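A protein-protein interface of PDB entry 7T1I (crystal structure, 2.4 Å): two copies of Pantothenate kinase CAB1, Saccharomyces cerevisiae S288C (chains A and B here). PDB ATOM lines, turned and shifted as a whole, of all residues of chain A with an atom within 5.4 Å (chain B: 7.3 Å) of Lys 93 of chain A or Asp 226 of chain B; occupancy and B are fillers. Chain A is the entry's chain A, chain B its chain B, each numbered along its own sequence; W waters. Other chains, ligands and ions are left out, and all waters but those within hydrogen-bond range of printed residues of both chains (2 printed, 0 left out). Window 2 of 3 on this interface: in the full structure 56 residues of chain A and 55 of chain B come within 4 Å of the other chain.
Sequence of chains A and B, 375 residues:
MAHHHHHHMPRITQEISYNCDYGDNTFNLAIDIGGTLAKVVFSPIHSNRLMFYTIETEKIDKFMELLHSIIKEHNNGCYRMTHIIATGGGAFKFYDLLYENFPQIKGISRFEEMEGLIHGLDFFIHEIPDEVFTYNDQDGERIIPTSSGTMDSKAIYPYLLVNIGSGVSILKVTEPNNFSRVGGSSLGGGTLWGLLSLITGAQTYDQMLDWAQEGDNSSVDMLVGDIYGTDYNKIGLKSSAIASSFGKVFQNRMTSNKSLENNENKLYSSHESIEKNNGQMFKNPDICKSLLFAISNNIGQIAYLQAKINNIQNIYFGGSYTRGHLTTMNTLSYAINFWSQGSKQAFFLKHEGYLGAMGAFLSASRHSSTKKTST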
ATOM      1  N   GLY A  89      27.777  -5.159  14.011  1.00  0.00           N
ATOM      2  CA  GLY A  89      27.954  -4.797  12.614  1.00  0.00           C
ATOM      3  C   GLY A  89      27.364  -3.422  12.321  1.00  0.00           C
ATOM      4  O   GLY A  89      27.934  -2.659  11.545  1.00  0.00           O
ATOM      5  N   GLY A  90      26.201  -3.137  12.927  1.00  0.00           N
ATOM      6  CA  GLY A  90      25.474  -1.903  12.663  1.00  0.00           C
ATOM      7  C   GLY A  90      26.228  -0.604  12.992  1.00  0.00           C
ATOM      8  O   GLY A  90      25.899   0.426  12.402  1.00  0.00           O
ATOM      9  N   ALA A  91      27.216  -0.660  13.916  1.00  0.00           N
ATOM     10  CA  ALA A  91      28.096   0.454  14.282  1.00  0.00           C
ATOM     11  C   ALA A  91      28.812   1.012  13.054  1.00  0.00           C
ATOM     12  O   ALA A  91      29.235   2.169  13.059  1.00  0.00           O
ATOM     13  CB  ALA A  91      29.123   0.047  15.324  1.00  0.00           C
ATOM     14  N   PHE A  92      29.032   0.148  12.052  1.00  0.00           N
ATOM     15  CA  PHE A  92      29.570   0.566  10.774  1.00  0.00           C
ATOM     16  C   PHE A  92      28.403   0.805   9.837  1.00  0.00           C
ATOM     17  O   PHE A  92      28.279   1.893   9.292  1.00  0.00           O
ATOM     18  CB  PHE A  92      30.620  -0.423  10.260  1.00  0.00           C
ATOM     19  CG  PHE A  92      31.888  -0.360  11.071  1.00  0.00           C
ATOM     20  CD1 PHE A  92      32.908   0.511  10.738  1.00  0.00           C
ATOM     21  CD2 PHE A  92      32.035  -1.120  12.232  1.00  0.00           C
ATOM     22  CE1 PHE A  92      34.074   0.580  11.501  1.00  0.00           C
ATOM     23  CE2 PHE A  92      33.197  -1.048  12.993  1.00  0.00           C
ATOM     24  CZ  PHE A  92      34.217  -0.203  12.624  1.00  0.00           C
ATOM     25  N   LYS A  93      27.540  -0.213   9.714  1.00  0.00           N
ATOM     26  CA  LYS A  93      26.551  -0.277   8.647  1.00  0.00           C
ATOM     27  C   LYS A  93      25.526   0.853   8.773  1.00  0.00           C
ATOM     28  O   LYS A  93      25.078   1.381   7.764  1.00  0.00           O
ATOM     29  CB  LYS A  93      25.843  -1.635   8.656  1.00  0.00           C
ATOM     30  CG  LYS A  93      24.755  -1.764   7.600  1.00  0.00           C
ATOM     31  CD  LYS A  93      23.944  -3.030   7.660  1.00  0.00           C
ATOM     32  CE  LYS A  93      22.996  -3.160   6.483  1.00  0.00           C
ATOM     33  NZ  LYS A  93      22.165  -4.385   6.599  1.00  0.00           N
ATOM     34  N   PHE A  94      25.141   1.197  10.007  1.00  0.00           N
ATOM     35  CA  PHE A  94      24.104   2.190  10.253  1.00  0.00           C
ATOM     36  C   PHE A  94      24.694   3.468  10.865  1.00  0.00           C
ATOM     37  O   PHE A  94      23.946   4.337  11.300  1.00  0.00           O
ATOM     38  CB  PHE A  94      23.028   1.614  11.181  1.00  0.00           C
ATOM     39  CG  PHE A  94      22.196   0.544  10.536  1.00  0.00           C
ATOM     40  CD1 PHE A  94      21.549   0.787   9.334  1.00  0.00           C
ATOM     41  CD2 PHE A  94      22.139  -0.735  11.078  1.00  0.00           C
ATOM     42  CE1 PHE A  94      20.820  -0.215   8.713  1.00  0.00           C
ATOM     43  CE2 PHE A  94      21.398  -1.735  10.460  1.00  0.00           C
ATOM     44  CZ  PHE A  94      20.731  -1.470   9.281  1.00  0.00           C
ATOM     45  N   TYR A  95      26.023   3.596  10.872  1.00  0.00           N
ATOM     46  CA  TYR A  95      26.657   4.744  11.486  1.00  0.00           C
ATOM     47  C   TYR A  95      26.177   6.053  10.852  1.00  0.00           C
ATOM     48  O   TYR A  95      25.774   6.975  11.559  1.00  0.00           O
ATOM     49  CB  TYR A  95      28.178   4.602  11.474  1.00  0.00           C
ATOM     50  CG  TYR A  95      28.874   5.676  12.278  1.00  0.00           C
ATOM     51  CD1 TYR A  95      29.193   5.478  13.616  1.00  0.00           C
ATOM     52  CD2 TYR A  95      29.160   6.912  11.708  1.00  0.00           C
ATOM     53  CE1 TYR A  95      29.856   6.449  14.343  1.00  0.00           C
ATOM     54  CE2 TYR A  95      29.785   7.908  12.430  1.00  0.00           C
ATOM     55  CZ  TYR A  95      30.145   7.669  13.747  1.00  0.00           C
ATOM     56  OH  TYR A  95      30.757   8.669  14.451  1.00  0.00           O
ATOM     57  N   ASP A  96      26.233   6.147   9.516  1.00  0.00           N
ATOM     58  CA  ASP A  96      25.767   7.347   8.835  1.00  0.00           C
ATOM     59  C   ASP A  96      24.332   7.680   9.243  1.00  0.00           C
ATOM     60  O   ASP A  96      24.025   8.820   9.580  1.00  0.00           O
ATOM     61  CB  ASP A  96      25.929   7.259   7.310  1.00  0.00           C
ATOM     62  CG  ASP A  96      27.374   7.130   6.852  1.00  0.00           C
ATOM     63  OD1 ASP A  96      28.264   7.673   7.552  1.00  0.00           O
ATOM     64  OD2 ASP A  96      27.609   6.411   5.844  1.00  0.00           O
ATOM     65  N   SER B 218      22.881 -16.964  -0.296  1.00  0.00           N
ATOM     66  CA  SER B 218      22.721 -15.669   0.363  1.00  0.00           C
ATOM     67  C   SER B 218      21.254 -15.259   0.408  1.00  0.00           C
ATOM     68  O   SER B 218      20.856 -14.435   1.222  1.00  0.00           O
ATOM     69  CB  SER B 218      23.557 -14.605  -0.272  1.00  0.00           C
ATOM     70  OG  SER B 218      23.154 -14.405  -1.607  1.00  0.00           O
ATOM     71  N   ASP B 221      20.889 -17.269   3.675  1.00  0.00           N
ATOM     72  CA  ASP B 221      21.938 -17.092   4.663  1.00  0.00           C
ATOM     73  C   ASP B 221      22.260 -15.610   4.863  1.00  0.00           C
ATOM     74  O   ASP B 221      22.499 -14.872   3.913  1.00  0.00           O
ATOM     75  CB  ASP B 221      23.251 -17.770   4.287  1.00  0.00           C
ATOM     76  CG  ASP B 221      23.146 -19.262   4.106  1.00  0.00           C
ATOM     77  OD1 ASP B 221      22.158 -19.838   4.601  1.00  0.00           O
ATOM     78  OD2 ASP B 221      24.056 -19.814   3.453  1.00  0.00           O
ATOM     79  N   MET B 222      22.323 -15.234   6.135  1.00  0.00           N
ATOM     80  CA  MET B 222      22.905 -13.990   6.579  1.00  0.00           C
ATOM     81  C   MET B 222      24.427 -14.091   6.461  1.00  0.00           C
ATOM     82  O   MET B 222      25.026 -15.012   7.023  1.00  0.00           O
ATOM     83  CB  MET B 222      22.481 -13.766   8.028  1.00  0.00           C
ATOM     84  CG  MET B 222      22.691 -12.351   8.496  1.00  0.00           C
ATOM     85  SD  MET B 222      21.792 -12.128  10.047  1.00  0.00           S
ATOM     86  CE  MET B 222      20.196 -11.703   9.340  1.00  0.00           C
ATOM     87  N   LEU B 223      25.028 -13.169   5.678  1.00  0.00           N
ATOM     88  CA  LEU B 223      26.473 -13.055   5.508  1.00  0.00           C
ATOM     89  C   LEU B 223      27.011 -11.930   6.379  1.00  0.00           C
ATOM     90  O   LEU B 223      26.252 -11.058   6.822  1.00  0.00           O
ATOM     91  CB  LEU B 223      26.824 -12.752   4.047  1.00  0.00           C
ATOM     92  CG  LEU B 223      26.071 -13.563   2.990  1.00  0.00           C
ATOM     93  CD1 LEU B 223      26.610 -13.256   1.588  1.00  0.00           C
ATOM     94  CD2 LEU B 223      26.167 -15.060   3.284  1.00  0.00           C
ATOM     95  N   VAL B 224      28.338 -11.949   6.560  1.00  0.00           N
ATOM     96  CA  VAL B 224      29.043 -10.943   7.340  1.00  0.00           C
ATOM     97  C   VAL B 224      28.681  -9.576   6.777  1.00  0.00           C
ATOM     98  O   VAL B 224      28.325  -8.670   7.532  1.00  0.00           O
ATOM     99  CB  VAL B 224      30.568 -11.160   7.366  1.00  0.00           C
ATOM    100  CG1 VAL B 224      31.316  -9.968   7.963  1.00  0.00           C
ATOM    101  CG2 VAL B 224      30.948 -12.448   8.091  1.00  0.00           C
ATOM    102  N   GLY B 225      28.755  -9.461   5.444  1.00  0.00           N
ATOM    103  CA  GLY B 225      28.451  -8.231   4.722  1.00  0.00           C
ATOM    104  C   GLY B 225      27.042  -7.695   5.003  1.00  0.00           C
ATOM    105  O   GLY B 225      26.849  -6.481   5.001  1.00  0.00           O
ATOM    106  N   ASP B 226      26.085  -8.598   5.284  1.00  0.00           N
ATOM    107  CA  ASP B 226      24.754  -8.203   5.697  1.00  0.00           C
ATOM    108  C   ASP B 226      24.757  -7.545   7.084  1.00  0.00           C
ATOM    109  O   ASP B 226      23.862  -6.771   7.402  1.00  0.00           O
ATOM    110  CB  ASP B 226      23.788  -9.381   5.682  1.00  0.00           C
ATOM    111  CG  ASP B 226      23.678 -10.082   4.339  1.00  0.00           C
ATOM    112  OD1 ASP B 226      23.468  -9.412   3.344  1.00  0.00           O
ATOM    113  OD2 ASP B 226      23.760 -11.295   4.315  1.00  0.00           O
ATOM    114  N   ILE B 227      25.736  -7.861   7.936  1.00  0.00           N
ATOM    115  CA  ILE B 227      25.684  -7.416   9.316  1.00  0.00           C
ATOM    116  C   ILE B 227      26.542  -6.158   9.485  1.00  0.00           C
ATOM    117  O   ILE B 227      26.179  -5.253  10.241  1.00  0.00           O
ATOM    118  CB  ILE B 227      26.160  -8.552  10.250  1.00  0.00           C
ATOM    119  CG1 ILE B 227      25.290  -9.807  10.119  1.00  0.00           C
ATOM    120  CG2 ILE B 227      26.305  -8.074  11.696  1.00  0.00           C
ATOM    121  CD1 ILE B 227      25.785 -11.026  10.893  1.00  0.00           C
ATOM    122  N   TYR B 228      27.687  -6.132   8.786  1.00  0.00           N
ATOM    123  CA  TYR B 228      28.724  -5.124   8.959  1.00  0.00           C
ATOM    124  C   TYR B 228      28.751  -4.117   7.803  1.00  0.00           C
ATOM    125  O   TYR B 228      29.398  -3.068   7.914  1.00  0.00           O
ATOM    126  CB  TYR B 228      30.083  -5.810   9.115  1.00  0.00           C
ATOM    127  CG  TYR B 228      30.469  -6.010  10.554  1.00  0.00           C
ATOM    128  CD1 TYR B 228      30.044  -7.124  11.269  1.00  0.00           C
ATOM    129  CD2 TYR B 228      31.209  -5.041  11.214  1.00  0.00           C
ATOM    130  CE1 TYR B 228      30.373  -7.281  12.606  1.00  0.00           C
ATOM    131  CE2 TYR B 228      31.551  -5.190  12.550  1.00  0.00           C
ATOM    132  CZ  TYR B 228      31.114  -6.301  13.255  1.00  0.00           C
ATOM    133  OH  TYR B 228      31.455  -6.418  14.579  1.00  0.00           O
ATOM    134  N   GLY B 229      28.062  -4.440   6.696  1.00  0.00           N
ATOM    135  CA  GLY B 229      28.173  -3.681   5.458  1.00  0.00           C
ATOM    136  C   GLY B 229      29.602  -3.686   4.898  1.00  0.00           C
ATOM    137  O   GLY B 229      29.901  -2.954   3.972  1.00  0.00           O
ATOM    138  N   THR B 230      30.482  -4.535   5.438  1.00  0.00           N
ATOM    139  CA  THR B 230      31.878  -4.557   5.050  1.00  0.00           C
ATOM    140  C   THR B 230      32.486  -5.853   5.576  1.00  0.00           C
ATOM    141  O   THR B 230      31.787  -6.626   6.215  1.00  0.00           O
ATOM    142  CB  THR B 230      32.597  -3.317   5.605  1.00  0.00           C
ATOM    143  OG1 THR B 230      33.897  -3.278   5.023  1.00  0.00           O
ATOM    144  CG2 THR B 230      32.701  -3.264   7.118  1.00  0.00           C
ATOM    145  N   SER B 239      33.117 -10.318   3.842  1.00  0.00           N
ATOM    146  CA  SER B 239      31.704  -9.983   3.839  1.00  0.00           C
ATOM    147  C   SER B 239      30.888 -11.169   3.335  1.00  0.00           C
ATOM    148  O   SER B 239      29.752 -11.352   3.764  1.00  0.00           O
ATOM    149  CB  SER B 239      31.423  -8.736   3.053  1.00  0.00           C
ATOM    150  OG  SER B 239      32.311  -8.663   1.965  1.00  0.00           O
ATOM    151  N   SER B 240      31.506 -11.993   2.478  1.00  0.00           N
ATOM    152  CA  SER B 240      30.800 -13.124   1.891  1.00  0.00           C
ATOM    153  C   SER B 240      30.759 -14.356   2.811  1.00  0.00           C
ATOM    154  O   SER B 240      29.985 -15.259   2.547  1.00  0.00           O
ATOM    155  CB  SER B 240      31.346 -13.451   0.520  1.00  0.00           C
ATOM    156  OG  SER B 240      32.696 -13.873   0.638  1.00  0.00           O
ATOM    157  N   ALA B 241      31.542 -14.403   3.899  1.00  0.00           N
ATOM    158  CA  ALA B 241      31.439 -15.487   4.869  1.00  0.00           C
ATOM    159  C   ALA B 241      30.023 -15.587   5.435  1.00  0.00           C
ATOM    160  O   ALA B 241      29.356 -14.564   5.631  1.00  0.00           O
ATOM    161  CB  ALA B 241      32.445 -15.333   5.976  1.00  0.00           C
ATOM    162  N   ALA B 243      27.491 -16.096   8.184  1.00  0.00           N
ATOM    163  CA  ALA B 243      27.410 -15.827   9.602  1.00  0.00           C
ATOM    164  C   ALA B 243      26.364 -16.751  10.222  1.00  0.00           C
ATOM    165  O   ALA B 243      26.578 -17.315  11.289  1.00  0.00           O
ATOM    166  CB  ALA B 243      27.095 -14.366   9.811  1.00  0.00           C
ATOM    167  N   LYS B 248      18.394 -15.574   7.338  1.00  0.00           N
ATOM    168  CA  LYS B 248      17.433 -14.662   6.733  1.00  0.00           C
ATOM    169  C   LYS B 248      16.014 -15.242   6.736  1.00  0.00           C
ATOM    170  O   LYS B 248      15.074 -14.549   6.355  1.00  0.00           O
ATOM    171  CB  LYS B 248      17.813 -14.313   5.290  1.00  0.00           C
ATOM    172  CG  LYS B 248      18.966 -13.336   5.130  1.00  0.00           C
ATOM    173  CD  LYS B 248      19.286 -13.024   3.686  1.00  0.00           C
ATOM    174  CE  LYS B 248      20.237 -11.856   3.571  1.00  0.00           C
ATOM    175  NZ  LYS B 248      21.486 -12.207   2.853  1.00  0.00           N
HETATM  176  O   HOH W   1      21.545  -5.246   9.107  1.00  0.00           O
HETATM  177  O   HOH W   2      24.772  -4.820   4.572  1.00  0.00           O
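Among the printed residues, merely in contact across the chains: Gly 89 of chain A with Tyr 228 of chain B (3.4 Å), Phe 92 of chain A with Tyr 228 of chain B (3.7 Å), Lys 93 of chain A with Tyr 228 of chain B (3.9 Å) and Lys 93 of chain A with Ile 227 of chain B (3.96 Å).
N of Leu 223 of chain B lies within hydrogen-bond range of OD2 of Asp 226 of chain B (2.6 Å).
The side-chain amino group of Lys 248 of chain B lies within salt-bridge range of the side-chain carboxylate of Asp 226 of chain B, 2.9 Å away.
Of the printed residues of chain B, Lys 93 of chain A touches Asp 226 (3.0 Å), Ile 227 (3.96 Å) and Tyr 228 (3.9 Å).
Leu 223 of chain B touches none of the printed residues of chain A.
Of chain A, only Lys 93 (3.0 Å) comes within 4 Å of Asp 226 of chain B.
Printed residues of chain A within 4 Å of Ile 227 of chain B: Gly 89, Gly 90 and Lys 93.
Of the printed residues of chain A, Tyr 228 of chain B touches Gly 89 (3.4 Å), Phe 92 (3.7 Å) and Lys 93 (3.9 Å).
The nearest printed residue of chain A that does not touch Asp 226 of chain B is Phe 94 of chain A (6.4 Å).
No position is printed for both chains.
Hydrophobic or aromatic side chains of chain B that line the printed part of chain A: Ile 227 and Tyr 228.
Among the printed residues, no Asp or Glu carboxylate lies within 4 Å of a Lys or Arg side-chain nitrogen of the other chain.
Water W2 bridges the backbone carbonyl oxygen of Gly 225 of chain B (2.7 Å) and the side-chain amino group of Lys 93 of chain A (3.3 Å).
Water W1 lies within hydrogen-bond range of the side-chain amino group (NZ) of Lys 93 of chain A (2.7 Å) and the backbone carbonyl oxygen (O) of Asp 226 of chain B (3.3 Å).
The backbone carbonyl oxygen of Ile 227 of chain B sits at hydrogen-bond distance from the backbone NH of Gly 90 of chain A, at 3.4 Å.
The side-chain amino group (NZ) of Lys 93 of chain A sits at hydrogen-bond distance from the backbone carbonyl oxygen (O) of Asp 226 of chain B, at 3.0 Å.
The backbone carbonyl oxygen (O) of Ile 227 of chain B sits close to the backbone carbonyl oxygen (O) of Gly 89 of chain A, 3.4 Å away.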
